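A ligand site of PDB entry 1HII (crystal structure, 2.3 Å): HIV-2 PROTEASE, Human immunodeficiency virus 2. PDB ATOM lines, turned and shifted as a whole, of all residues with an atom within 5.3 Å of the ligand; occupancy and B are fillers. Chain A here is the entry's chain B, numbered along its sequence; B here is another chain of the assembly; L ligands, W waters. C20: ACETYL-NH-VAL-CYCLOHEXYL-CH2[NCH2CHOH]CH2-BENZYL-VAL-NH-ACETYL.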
ATOM      1  N   ARG A   8      17.237  -0.923 -29.530  1.00  0.00           N
ATOM      2  CA  ARG A   8      18.398  -0.217 -29.001  1.00  0.00           C
ATOM      3  C   ARG A   8      18.796   0.874 -30.007  1.00  0.00           C
ATOM      4  O   ARG A   8      18.835   0.612 -31.224  1.00  0.00           O
ATOM      5  CB  ARG A   8      19.575  -1.171 -28.869  1.00  0.00           C
ATOM      6  CG  ARG A   8      19.426  -2.205 -27.783  1.00  0.00           C
ATOM      7  CD  ARG A   8      20.689  -2.984 -27.588  1.00  0.00           C
ATOM      8  NE  ARG A   8      20.567  -3.937 -26.482  1.00  0.00           N
ATOM      9  CZ  ARG A   8      21.465  -4.873 -26.187  1.00  0.00           C
ATOM     10  NH1 ARG A   8      22.559  -5.018 -26.914  1.00  0.00           N
ATOM     11  NH2 ARG A   8      21.314  -5.615 -25.085  1.00  0.00           N
ATOM     12  N   LEU A  23      26.129   2.317 -29.288  1.00  0.00           N
ATOM     13  CA  LEU A  23      24.844   2.455 -28.610  1.00  0.00           C
ATOM     14  C   LEU A  23      24.743   3.895 -28.046  1.00  0.00           C
ATOM     15  O   LEU A  23      25.633   4.311 -27.307  1.00  0.00           O
ATOM     16  CB  LEU A  23      24.811   1.441 -27.449  1.00  0.00           C
ATOM     17  CG  LEU A  23      23.673   1.488 -26.416  1.00  0.00           C
ATOM     18  CD1 LEU A  23      22.334   1.305 -27.111  1.00  0.00           C
ATOM     19  CD2 LEU A  23      23.869   0.403 -25.378  1.00  0.00           C
ATOM     20  N   ASP A  25      23.735   6.347 -25.503  1.00  0.00           N
ATOM     21  CA  ASP A  25      23.407   6.078 -24.130  1.00  0.00           C
ATOM     22  C   ASP A  25      23.327   7.251 -23.156  1.00  0.00           C
ATOM     23  O   ASP A  25      24.352   7.699 -22.590  1.00  0.00           O
ATOM     24  CB  ASP A  25      24.468   5.056 -23.700  1.00  0.00           C
ATOM     25  CG  ASP A  25      24.267   4.513 -22.325  1.00  0.00           C
ATOM     26  OD1 ASP A  25      23.303   4.867 -21.642  1.00  0.00           O
ATOM     27  OD2 ASP A  25      25.120   3.713 -21.923  1.00  0.00           O
ATOM     28  N   GLY A  27      22.332   7.045 -20.196  1.00  0.00           N
ATOM     29  CA  GLY A  27      22.668   6.585 -18.848  1.00  0.00           C
ATOM     30  C   GLY A  27      24.176   6.497 -18.669  1.00  0.00           C
ATOM     31  O   GLY A  27      24.647   6.025 -17.635  1.00  0.00           O
ATOM     32  N   ALA A  28      24.921   6.965 -19.669  1.00  0.00           N
ATOM     33  CA  ALA A  28      26.381   6.918 -19.596  1.00  0.00           C
ATOM     34  C   ALA A  28      27.019   8.310 -19.526  1.00  0.00           C
ATOM     35  O   ALA A  28      26.667   9.195 -20.300  1.00  0.00           O
ATOM     36  CB  ALA A  28      26.922   6.148 -20.788  1.00  0.00           C
ATOM     37  N   ASP A  29      27.953   8.504 -18.599  1.00  0.00           N
ATOM     38  CA  ASP A  29      28.602   9.808 -18.511  1.00  0.00           C
ATOM     39  C   ASP A  29      29.675   9.958 -19.580  1.00  0.00           C
ATOM     40  O   ASP A  29      29.853  11.039 -20.152  1.00  0.00           O
ATOM     41  CB  ASP A  29      29.269   9.990 -17.152  1.00  0.00           C
ATOM     42  CG  ASP A  29      28.281   9.991 -15.987  1.00  0.00           C
ATOM     43  OD1 ASP A  29      27.093  10.339 -16.147  1.00  0.00           O
ATOM     44  OD2 ASP A  29      28.736   9.686 -14.875  1.00  0.00           O
ATOM     45  N   ASP A  30      30.362   8.849 -19.857  1.00  0.00           N
ATOM     46  CA  ASP A  30      31.481   8.774 -20.817  1.00  0.00           C
ATOM     47  C   ASP A  30      31.158   7.870 -21.982  1.00  0.00           C
ATOM     48  O   ASP A  30      30.172   7.138 -21.967  1.00  0.00           O
ATOM     49  CB  ASP A  30      32.714   8.172 -20.115  1.00  0.00           C
ATOM     50  CG  ASP A  30      33.014   8.821 -18.791  1.00  0.00           C
ATOM     51  OD1 ASP A  30      33.202  10.055 -18.763  1.00  0.00           O
ATOM     52  OD2 ASP A  30      33.011   8.110 -17.782  1.00  0.00           O
ATOM     53  N   ILE A  32      32.754   4.736 -24.346  1.00  0.00           N
ATOM     54  CA  ILE A  32      33.728   3.679 -24.276  1.00  0.00           C
ATOM     55  C   ILE A  32      33.575   2.804 -25.512  1.00  0.00           C
ATOM     56  O   ILE A  32      32.507   2.271 -25.778  1.00  0.00           O
ATOM     57  CB  ILE A  32      33.527   2.838 -23.004  1.00  0.00           C
ATOM     58  CG1 ILE A  32      33.415   3.769 -21.806  1.00  0.00           C
ATOM     59  CG2 ILE A  32      34.690   1.847 -22.799  1.00  0.00           C
ATOM     60  CD1 ILE A  32      33.258   3.052 -20.515  1.00  0.00           C
ATOM     61  N   VAL A  47      36.208   3.059 -14.868  1.00  0.00           N
ATOM     62  CA  VAL A  47      34.822   3.406 -15.048  1.00  0.00           C
ATOM     63  C   VAL A  47      33.996   2.292 -14.422  1.00  0.00           C
ATOM     64  O   VAL A  47      34.373   1.124 -14.490  1.00  0.00           O
ATOM     65  CB  VAL A  47      34.487   3.597 -16.559  1.00  0.00           C
ATOM     66  CG1 VAL A  47      32.979   3.713 -16.784  1.00  0.00           C
ATOM     67  CG2 VAL A  47      35.179   4.878 -17.072  1.00  0.00           C
ATOM     68  N   GLY A  48      32.935   2.672 -13.712  1.00  0.00           N
ATOM     69  CA  GLY A  48      32.074   1.690 -13.101  1.00  0.00           C
ATOM     70  C   GLY A  48      30.682   1.709 -13.702  1.00  0.00           C
ATOM     71  O   GLY A  48      30.236   2.706 -14.260  1.00  0.00           O
ATOM     72  N   GLY A  49      30.052   0.540 -13.678  1.00  0.00           N
ATOM     73  CA  GLY A  49      28.690   0.395 -14.162  1.00  0.00           C
ATOM     74  C   GLY A  49      28.027  -0.686 -13.322  1.00  0.00           C
ATOM     75  O   GLY A  49      28.343  -0.877 -12.155  1.00  0.00           O
ATOM     76  N   ILE A  50      27.069  -1.380 -13.915  1.00  0.00           N
ATOM     77  CA  ILE A  50      26.387  -2.489 -13.244  1.00  0.00           C
ATOM     78  C   ILE A  50      27.479  -3.549 -13.195  1.00  0.00           C
ATOM     79  O   ILE A  50      28.337  -3.598 -14.097  1.00  0.00           O
ATOM     80  CB  ILE A  50      25.198  -2.970 -14.139  1.00  0.00           C
ATOM     81  CG1 ILE A  50      23.981  -2.078 -13.967  1.00  0.00           C
ATOM     82  CG2 ILE A  50      24.921  -4.452 -13.975  1.00  0.00           C
ATOM     83  CD1 ILE A  50      23.400  -2.060 -12.609  1.00  0.00           C
ATOM     84  N   THR A  80      34.787  -3.511 -23.437  1.00  0.00           N
ATOM     85  CA  THR A  80      33.364  -3.356 -23.237  1.00  0.00           C
ATOM     86  C   THR A  80      32.662  -4.274 -24.221  1.00  0.00           C
ATOM     87  O   THR A  80      33.103  -4.431 -25.370  1.00  0.00           O
ATOM     88  CB  THR A  80      32.907  -1.884 -23.456  1.00  0.00           C
ATOM     89  OG1 THR A  80      31.490  -1.799 -23.329  1.00  0.00           O
ATOM     90  CG2 THR A  80      33.320  -1.375 -24.836  1.00  0.00           C
ATOM     91  N   PRO A  81      31.540  -4.889 -23.808  1.00  0.00           N
ATOM     92  CA  PRO A  81      30.788  -5.799 -24.680  1.00  0.00           C
ATOM     93  C   PRO A  81      30.124  -5.012 -25.807  1.00  0.00           C
ATOM     94  O   PRO A  81      30.005  -5.504 -26.928  1.00  0.00           O
ATOM     95  CB  PRO A  81      29.735  -6.367 -23.756  1.00  0.00           C
ATOM     96  CG  PRO A  81      30.258  -6.107 -22.353  1.00  0.00           C
ATOM     97  CD  PRO A  81      30.903  -4.784 -22.485  1.00  0.00           C
ATOM     98  N   ILE A  82      29.740  -3.776 -25.523  1.00  0.00           N
ATOM     99  CA  ILE A  82      29.095  -2.945 -26.537  1.00  0.00           C
ATOM    100  C   ILE A  82      29.768  -1.575 -26.525  1.00  0.00           C
ATOM    101  O   ILE A  82      30.188  -1.121 -25.461  1.00  0.00           O
ATOM    102  CB  ILE A  82      27.560  -2.757 -26.225  1.00  0.00           C
ATOM    103  CG1 ILE A  82      26.878  -4.117 -26.029  1.00  0.00           C
ATOM    104  CG2 ILE A  82      26.843  -2.120 -27.397  1.00  0.00           C
ATOM    105  CD1 ILE A  82      25.376  -4.020 -25.791  1.00  0.00           C
ATOM    106  N   ILE A  84      29.782   2.353 -26.499  1.00  0.00           N
ATOM    107  CA  ILE A  84      28.837   3.312 -25.972  1.00  0.00           C
ATOM    108  C   ILE A  84      29.232   4.775 -26.231  1.00  0.00           C
ATOM    109  O   ILE A  84      30.393   5.158 -26.015  1.00  0.00           O
ATOM    110  CB  ILE A  84      28.761   3.177 -24.366  1.00  0.00           C
ATOM    111  CG1 ILE A  84      28.302   1.778 -23.939  1.00  0.00           C
ATOM    112  CG2 ILE A  84      27.906   4.287 -23.721  1.00  0.00           C
ATOM    113  CD1 ILE A  84      26.928   1.500 -24.413  1.00  0.00           C
ATOM    114  N   ARG B   8      22.858  14.576 -15.796  1.00  0.00           N
ATOM    115  CA  ARG B   8      22.231  13.243 -15.815  1.00  0.00           C
ATOM    116  C   ARG B   8      20.710  13.421 -15.818  1.00  0.00           C
ATOM    117  O   ARG B   8      20.175  14.187 -15.025  1.00  0.00           O
ATOM    118  CB  ARG B   8      22.697  12.454 -14.579  1.00  0.00           C
ATOM    119  CG  ARG B   8      23.703  11.396 -14.928  1.00  0.00           C
ATOM    120  CD  ARG B   8      24.928  11.346 -14.092  1.00  0.00           C
ATOM    121  NE  ARG B   8      24.759  10.552 -12.897  1.00  0.00           N
ATOM    122  CZ  ARG B   8      25.693   9.802 -12.327  1.00  0.00           C
ATOM    123  NH1 ARG B   8      26.909   9.691 -12.834  1.00  0.00           N
ATOM    124  NH2 ARG B   8      25.432   9.223 -11.153  1.00  0.00           N
ATOM    125  N   LEU B  23      17.251   7.304 -13.188  1.00  0.00           N
ATOM    126  CA  LEU B  23      17.979   7.801 -14.349  1.00  0.00           C
ATOM    127  C   LEU B  23      17.251   7.291 -15.590  1.00  0.00           C
ATOM    128  O   LEU B  23      17.007   6.092 -15.702  1.00  0.00           O
ATOM    129  CB  LEU B  23      19.425   7.232 -14.365  1.00  0.00           C
ATOM    130  CG  LEU B  23      20.357   7.502 -15.571  1.00  0.00           C
ATOM    131  CD1 LEU B  23      20.569   8.953 -15.664  1.00  0.00           C
ATOM    132  CD2 LEU B  23      21.708   6.861 -15.366  1.00  0.00           C
ATOM    133  N   ASP B  25      17.388   6.028 -18.907  1.00  0.00           N
ATOM    134  CA  ASP B  25      18.471   5.412 -19.638  1.00  0.00           C
ATOM    135  C   ASP B  25      18.156   4.722 -20.990  1.00  0.00           C
ATOM    136  O   ASP B  25      17.607   3.624 -21.009  1.00  0.00           O
ATOM    137  CB  ASP B  25      19.094   4.402 -18.671  1.00  0.00           C
ATOM    138  CG  ASP B  25      20.470   3.901 -19.090  1.00  0.00           C
ATOM    139  OD1 ASP B  25      20.977   4.163 -20.209  1.00  0.00           O
ATOM    140  OD2 ASP B  25      21.042   3.206 -18.242  1.00  0.00           O
ATOM    141  N   GLY B  27      20.420   3.425 -22.890  1.00  0.00           N
ATOM    142  CA  GLY B  27      21.328   2.301 -23.083  1.00  0.00           C
ATOM    143  C   GLY B  27      21.044   1.119 -22.160  1.00  0.00           C
ATOM    144  O   GLY B  27      21.923   0.306 -21.836  1.00  0.00           O
ATOM    145  N   ALA B  28      19.807   1.071 -21.652  1.00  0.00           N
ATOM    146  CA  ALA B  28      19.399  -0.057 -20.794  1.00  0.00           C
ATOM    147  C   ALA B  28      18.138  -0.709 -21.380  1.00  0.00           C
ATOM    148  O   ALA B  28      17.173  -0.010 -21.695  1.00  0.00           O
ATOM    149  CB  ALA B  28      19.125   0.401 -19.360  1.00  0.00           C
ATOM    150  N   ASP B  29      18.161  -2.032 -21.563  1.00  0.00           N
ATOM    151  CA  ASP B  29      16.979  -2.752 -22.059  1.00  0.00           C
ATOM    152  C   ASP B  29      15.947  -2.839 -20.937  1.00  0.00           C
ATOM    153  O   ASP B  29      14.761  -2.730 -21.206  1.00  0.00           O
ATOM    154  CB  ASP B  29      17.312  -4.196 -22.473  1.00  0.00           C
ATOM    155  CG  ASP B  29      18.340  -4.270 -23.596  1.00  0.00           C
ATOM    156  OD1 ASP B  29      18.526  -3.272 -24.327  1.00  0.00           O
ATOM    157  OD2 ASP B  29      18.972  -5.342 -23.728  1.00  0.00           O
ATOM    158  N   ASP B  30      16.417  -2.989 -19.704  1.00  0.00           N
ATOM    159  CA  ASP B  30      15.544  -3.133 -18.529  1.00  0.00           C
ATOM    160  C   ASP B  30      15.652  -2.012 -17.499  1.00  0.00           C
ATOM    161  O   ASP B  30      16.506  -1.125 -17.617  1.00  0.00           O
ATOM    162  CB  ASP B  30      15.834  -4.456 -17.808  1.00  0.00           C
ATOM    163  CG  ASP B  30      15.961  -5.618 -18.756  1.00  0.00           C
ATOM    164  OD1 ASP B  30      15.015  -5.856 -19.533  1.00  0.00           O
ATOM    165  OD2 ASP B  30      17.035  -6.262 -18.756  1.00  0.00           O
ATOM    166  N   ILE B  32      16.026  -1.268 -13.380  1.00  0.00           N
ATOM    167  CA  ILE B  32      16.480  -1.891 -12.159  1.00  0.00           C
ATOM    168  C   ILE B  32      16.522  -0.847 -11.058  1.00  0.00           C
ATOM    169  O   ILE B  32      17.032   0.274 -11.260  1.00  0.00           O
ATOM    170  CB  ILE B  32      17.826  -2.657 -12.349  1.00  0.00           C
ATOM    171  CG1 ILE B  32      18.510  -2.873 -11.012  1.00  0.00           C
ATOM    172  CG2 ILE B  32      18.693  -1.912 -13.291  1.00  0.00           C
ATOM    173  CD1 ILE B  32      19.045  -4.235 -10.781  1.00  0.00           C
ATOM    174  N   VAL B  47      21.296  -9.979 -14.816  1.00  0.00           N
ATOM    175  CA  VAL B  47      21.392  -8.842 -15.714  1.00  0.00           C
ATOM    176  C   VAL B  47      22.866  -8.465 -15.843  1.00  0.00           C
ATOM    177  O   VAL B  47      23.629  -8.524 -14.880  1.00  0.00           O
ATOM    178  CB  VAL B  47      20.468  -7.661 -15.258  1.00  0.00           C
ATOM    179  CG1 VAL B  47      21.052  -6.901 -14.101  1.00  0.00           C
ATOM    180  CG2 VAL B  47      20.202  -6.749 -16.422  1.00  0.00           C
ATOM    181  N   GLY B  48      23.280  -8.197 -17.075  1.00  0.00           N
ATOM    182  CA  GLY B  48      24.680  -7.848 -17.319  1.00  0.00           C
ATOM    183  C   GLY B  48      24.891  -6.404 -17.692  1.00  0.00           C
ATOM    184  O   GLY B  48      24.089  -5.819 -18.425  1.00  0.00           O
ATOM    185  N   GLY B  49      25.984  -5.833 -17.213  1.00  0.00           N
ATOM    186  CA  GLY B  49      26.315  -4.459 -17.487  1.00  0.00           C
ATOM    187  C   GLY B  49      27.760  -4.356 -17.895  1.00  0.00           C
ATOM    188  O   GLY B  49      28.357  -5.323 -18.367  1.00  0.00           O
ATOM    189  N   ILE B  50      28.376  -3.197 -17.650  1.00  0.00           N
ATOM    190  CA  ILE B  50      29.770  -3.032 -18.040  1.00  0.00           C
ATOM    191  C   ILE B  50      30.800  -3.790 -17.192  1.00  0.00           C
ATOM    192  O   ILE B  50      31.786  -4.282 -17.735  1.00  0.00           O
ATOM    193  CB  ILE B  50      30.146  -1.526 -18.258  1.00  0.00           C
ATOM    194  CG1 ILE B  50      31.003  -1.396 -19.494  1.00  0.00           C
ATOM    195  CG2 ILE B  50      30.899  -0.939 -17.085  1.00  0.00           C
ATOM    196  CD1 ILE B  50      31.437  -0.019 -19.704  1.00  0.00           C
ATOM    197  N   THR B  80      22.084  -2.003  -7.378  1.00  0.00           N
ATOM    198  CA  THR B  80      22.518  -1.075  -8.374  1.00  0.00           C
ATOM    199  C   THR B  80      22.840   0.233  -7.636  1.00  0.00           C
ATOM    200  O   THR B  80      22.188   0.588  -6.646  1.00  0.00           O
ATOM    201  CB  THR B  80      21.441  -0.875  -9.468  1.00  0.00           C
ATOM    202  OG1 THR B  80      21.852   0.178 -10.356  1.00  0.00           O
ATOM    203  CG2 THR B  80      20.070  -0.539  -8.848  1.00  0.00           C
ATOM    204  N   PRO B  81      23.904   0.921  -8.080  1.00  0.00           N
ATOM    205  CA  PRO B  81      24.354   2.185  -7.474  1.00  0.00           C
ATOM    206  C   PRO B  81      23.408   3.324  -7.782  1.00  0.00           C
ATOM    207  O   PRO B  81      23.330   4.303  -7.033  1.00  0.00           O
ATOM    208  CB  PRO B  81      25.691   2.428  -8.165  1.00  0.00           C
ATOM    209  CG  PRO B  81      26.070   1.075  -8.807  1.00  0.00           C
ATOM    210  CD  PRO B  81      24.751   0.536  -9.218  1.00  0.00           C
ATOM    211  N   ILE B  82      22.686   3.203  -8.901  1.00  0.00           N
ATOM    212  CA  ILE B  82      21.774   4.240  -9.369  1.00  0.00           C
ATOM    213  C   ILE B  82      20.545   3.516  -9.855  1.00  0.00           C
ATOM    214  O   ILE B  82      20.637   2.437 -10.430  1.00  0.00           O
ATOM    215  CB  ILE B  82      22.420   5.008 -10.615  1.00  0.00           C
ATOM    216  CG1 ILE B  82      23.803   5.521 -10.282  1.00  0.00           C
ATOM    217  CG2 ILE B  82      21.609   6.252 -11.029  1.00  0.00           C
ATOM    218  CD1 ILE B  82      24.441   6.229 -11.415  1.00  0.00           C
ATOM    219  N   ILE B  84      17.791   2.796 -12.374  1.00  0.00           N
ATOM    220  CA  ILE B  84      17.659   2.874 -13.823  1.00  0.00           C
ATOM    221  C   ILE B  84      16.240   2.553 -14.340  1.00  0.00           C
ATOM    222  O   ILE B  84      15.634   1.557 -13.964  1.00  0.00           O
ATOM    223  CB  ILE B  84      18.583   1.793 -14.502  1.00  0.00           C
ATOM    224  CG1 ILE B  84      20.062   1.953 -14.108  1.00  0.00           C
ATOM    225  CG2 ILE B  84      18.448   1.828 -15.999  1.00  0.00           C
ATOM    226  CD1 ILE B  84      20.612   3.270 -14.475  1.00  0.00           C
HETATM  227  C1  C20 L   1      29.031   5.948 -14.457  1.00  0.00           C
HETATM  228  C2  C20 L   1      28.577   5.590 -15.882  1.00  0.00           C
HETATM  229  O3  C20 L   1      28.098   6.452 -16.631  1.00  0.00           O
HETATM  230  N4  C20 L   1      28.732   4.320 -16.242  1.00  0.00           N
HETATM  231  C5  C20 L   1      28.222   3.815 -17.518  1.00  0.00           C
HETATM  232  C6  C20 L   1      29.389   3.364 -18.437  1.00  0.00           C
HETATM  233  C7  C20 L   1      28.873   2.795 -19.779  1.00  0.00           C
HETATM  234  C8  C20 L   1      30.332   4.562 -18.702  1.00  0.00           C
HETATM  235  C9  C20 L   1      27.181   2.685 -17.330  1.00  0.00           C
HETATM  236  O10 C20 L   1      27.543   1.550 -16.988  1.00  0.00           O
HETATM  237  N11 C20 L   1      25.907   3.017 -17.562  1.00  0.00           N
HETATM  238  C12 C20 L   1      24.811   2.060 -17.462  1.00  0.00           C
HETATM  239  C13 C20 L   1      23.898   2.442 -16.300  1.00  0.00           C
HETATM  240  C14 C20 L   1      24.645   2.674 -15.015  1.00  0.00           C
HETATM  241  C15 C20 L   1      25.366   3.956 -14.769  1.00  0.00           C
HETATM  242  C16 C20 L   1      26.058   4.098 -13.570  1.00  0.00           C
HETATM  243  C17 C20 L   1      26.079   3.074 -12.600  1.00  0.00           C
HETATM  244  C18 C20 L   1      25.406   1.859 -12.799  1.00  0.00           C
HETATM  245  C19 C20 L   1      24.688   1.621 -13.976  1.00  0.00           C
HETATM  246  C20 C20 L   1      23.975   1.986 -18.753  1.00  0.00           C
HETATM  247  O21 C20 L   1      23.618   3.284 -19.224  1.00  0.00           O
HETATM  248  C22 C20 L   1      24.733   1.407 -19.908  1.00  0.00           C
HETATM  249  N23 C20 L   1      24.865  -0.009 -19.824  1.00  0.00           N
HETATM  250  C24 C20 L   1      25.372  -0.378 -21.124  1.00  0.00           C
HETATM  251  C25 C20 L   1      25.773  -1.833 -21.035  1.00  0.00           C
HETATM  252  C26 C20 L   1      27.222  -2.037 -21.418  1.00  0.00           C
HETATM  253  C27 C20 L   1      27.602  -3.488 -21.366  1.00  0.00           C
HETATM  254  C28 C20 L   1      26.722  -4.280 -22.281  1.00  0.00           C
HETATM  255  C29 C20 L   1      25.257  -4.080 -21.949  1.00  0.00           C
HETATM  256  C30 C20 L   1      24.912  -2.633 -22.000  1.00  0.00           C
HETATM  257  N31 C20 L   1      23.562  -0.582 -19.545  1.00  0.00           N
HETATM  258  C32 C20 L   1      23.394  -1.502 -18.581  1.00  0.00           C
HETATM  259  O33 C20 L   1      24.246  -1.754 -17.716  1.00  0.00           O
HETATM  260  C34 C20 L   1      22.067  -2.264 -18.599  1.00  0.00           C
HETATM  261  N35 C20 L   1      22.217  -3.554 -19.269  1.00  0.00           N
HETATM  262  C36 C20 L   1      21.516  -2.432 -17.156  1.00  0.00           C
HETATM  263  C37 C20 L   1      21.480  -1.099 -16.416  1.00  0.00           C
HETATM  264  C38 C20 L   1      20.102  -2.998 -17.219  1.00  0.00           C
HETATM  265  C39 C20 L   1      21.571  -3.850 -20.392  1.00  0.00           C
HETATM  266  O40 C20 L   1      20.786  -3.068 -20.942  1.00  0.00           O
HETATM  267  C41 C20 L   1      21.785  -5.211 -21.024  1.00  0.00           C
HETATM  268  O   HOH W   1      25.311   8.031 -15.850  1.00  0.00           O
HETATM  269  O   HOH W   2      21.202  -1.603 -23.877  1.00  0.00           O
HETATM  270  O   HOH W   3      32.140   5.494 -13.037  1.00  0.00           O
HETATM  271  O   HOH W   4      26.773  -0.902 -16.680  1.00  0.00           O
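O21 of the ligand sits at hydrogen-bond distance from OD2 of Asp 25 of chain B, at 2.8 Å. The backbone NH of Asp 29 of chain A is in hydrogen-bond range of an oxygen (O3) of the ligand (2.8 Å). An oxygen (O40) of the ligand lies within hydrogen-bond range of the backbone NH (N) of Asp 29 of chain B. The side-chain carboxylate (OD1) of Asp 25 of chain A is in hydrogen-bond range of an oxygen (O21) of the ligand, at 2.9 Å. O of Gly 27 of chain B lies within hydrogen-bond range of N31 of the ligand (3.0 Å). The backbone carbonyl oxygen of Gly 48 of chain A sits at hydrogen-bond distance from a nitrogen (N4) of the ligand. The backbone carbonyl oxygen of Gly 48 of chain B sits at hydrogen-bond distance from a nitrogen (N35) of the ligand, at 3.1 Å. N11 of the ligand sits at hydrogen-bond distance from O of Gly 27 of chain A, at 3.3 Å.
The side-chain carboxylate (OD1) of Asp 25 of chain B lies within hydrogen-bond range of the backbone NH (N) of Gly 27 of chain B. The side-chain carboxylate (OD1) of Asp 25 of chain B sits at hydrogen-bond distance from the backbone NH (N) of Gly 27 of chain A (3.2 Å). The side-chain carboxylate of Asp 29 of chain A lies within salt-bridge range of the guanidinium group of Arg 8 of chain B (2.7 Å). OD2 of Asp 29 of chain B lies within salt-bridge range of NH2 of Arg 8 of chain A (2.7 Å). OD1 of Asp 25 of chain A lies within hydrogen-bond range of N of Gly 27 of chain B (3.5 Å). N of Ala 28 of chain A sits at hydrogen-bond distance from OD1 of Asp 25 of chain A, at 3.3 Å. The backbone carbonyl oxygen (O) of Ile 82 of chain B lies within hydrogen-bond range of the side-chain hydroxyl (OG1) of Thr 80 of chain B (2.6 Å). N of Ile 84 of chain A is in hydrogen-bond range of O of Ile 32 of chain A (2.8 Å).
Residues that only touch the ligand: Gly 49 of chain A (3.3 Å), Ala 28 of chain B (3.3 Å), Val 47 of chain A (3.4 Å), Gly 49 of chain B (3.4 Å), Ile 82 of chain B (3.4 Å), Ala 28 of chain A (3.5 Å), Ile 50 of chain A (3.6 Å), Pro 81 of chain A (3.7 Å), Ile 82 of chain A (3.8 Å), Ile 32 of chain A (3.8 Å), Ile 50 of chain B (3.8 Å), Val 47 of chain B (3.8 Å), Ile 84 of chain B (3.8 Å) and Pro 81 of chain B (3.9 Å). 22 residues have an atom within 4 Å of the ligand: Asp 25 of chain A, Gly 27 of chain A, Ala 28 of chain A, Asp 29 of chain A, Ile 32 of chain A, Val 47 of chain A, Gly 48 of chain A, Gly 49 of chain A, Ile 50 of chain A, Pro 81 of chain A, Ile 82 of chain A, Asp 25 of chain B, Gly 27 of chain B, Ala 28 of chain B, Asp 29 of chain B, Val 47 of chain B, Gly 48 of chain B, Gly 49 of chain B, Ile 50 of chain B, Pro 81 of chain B, Ile 82 of chain B and Ile 84 of chain B. Along chain A the residues within 4 Å of the ligand span positions 25 to 82.
Water W4 lies within hydrogen-bond range of O10 of the ligand (2.6 Å), N of Ile 50 of chain A (2.8 Å) and N of Ile 50 of chain B (3.0 Å).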
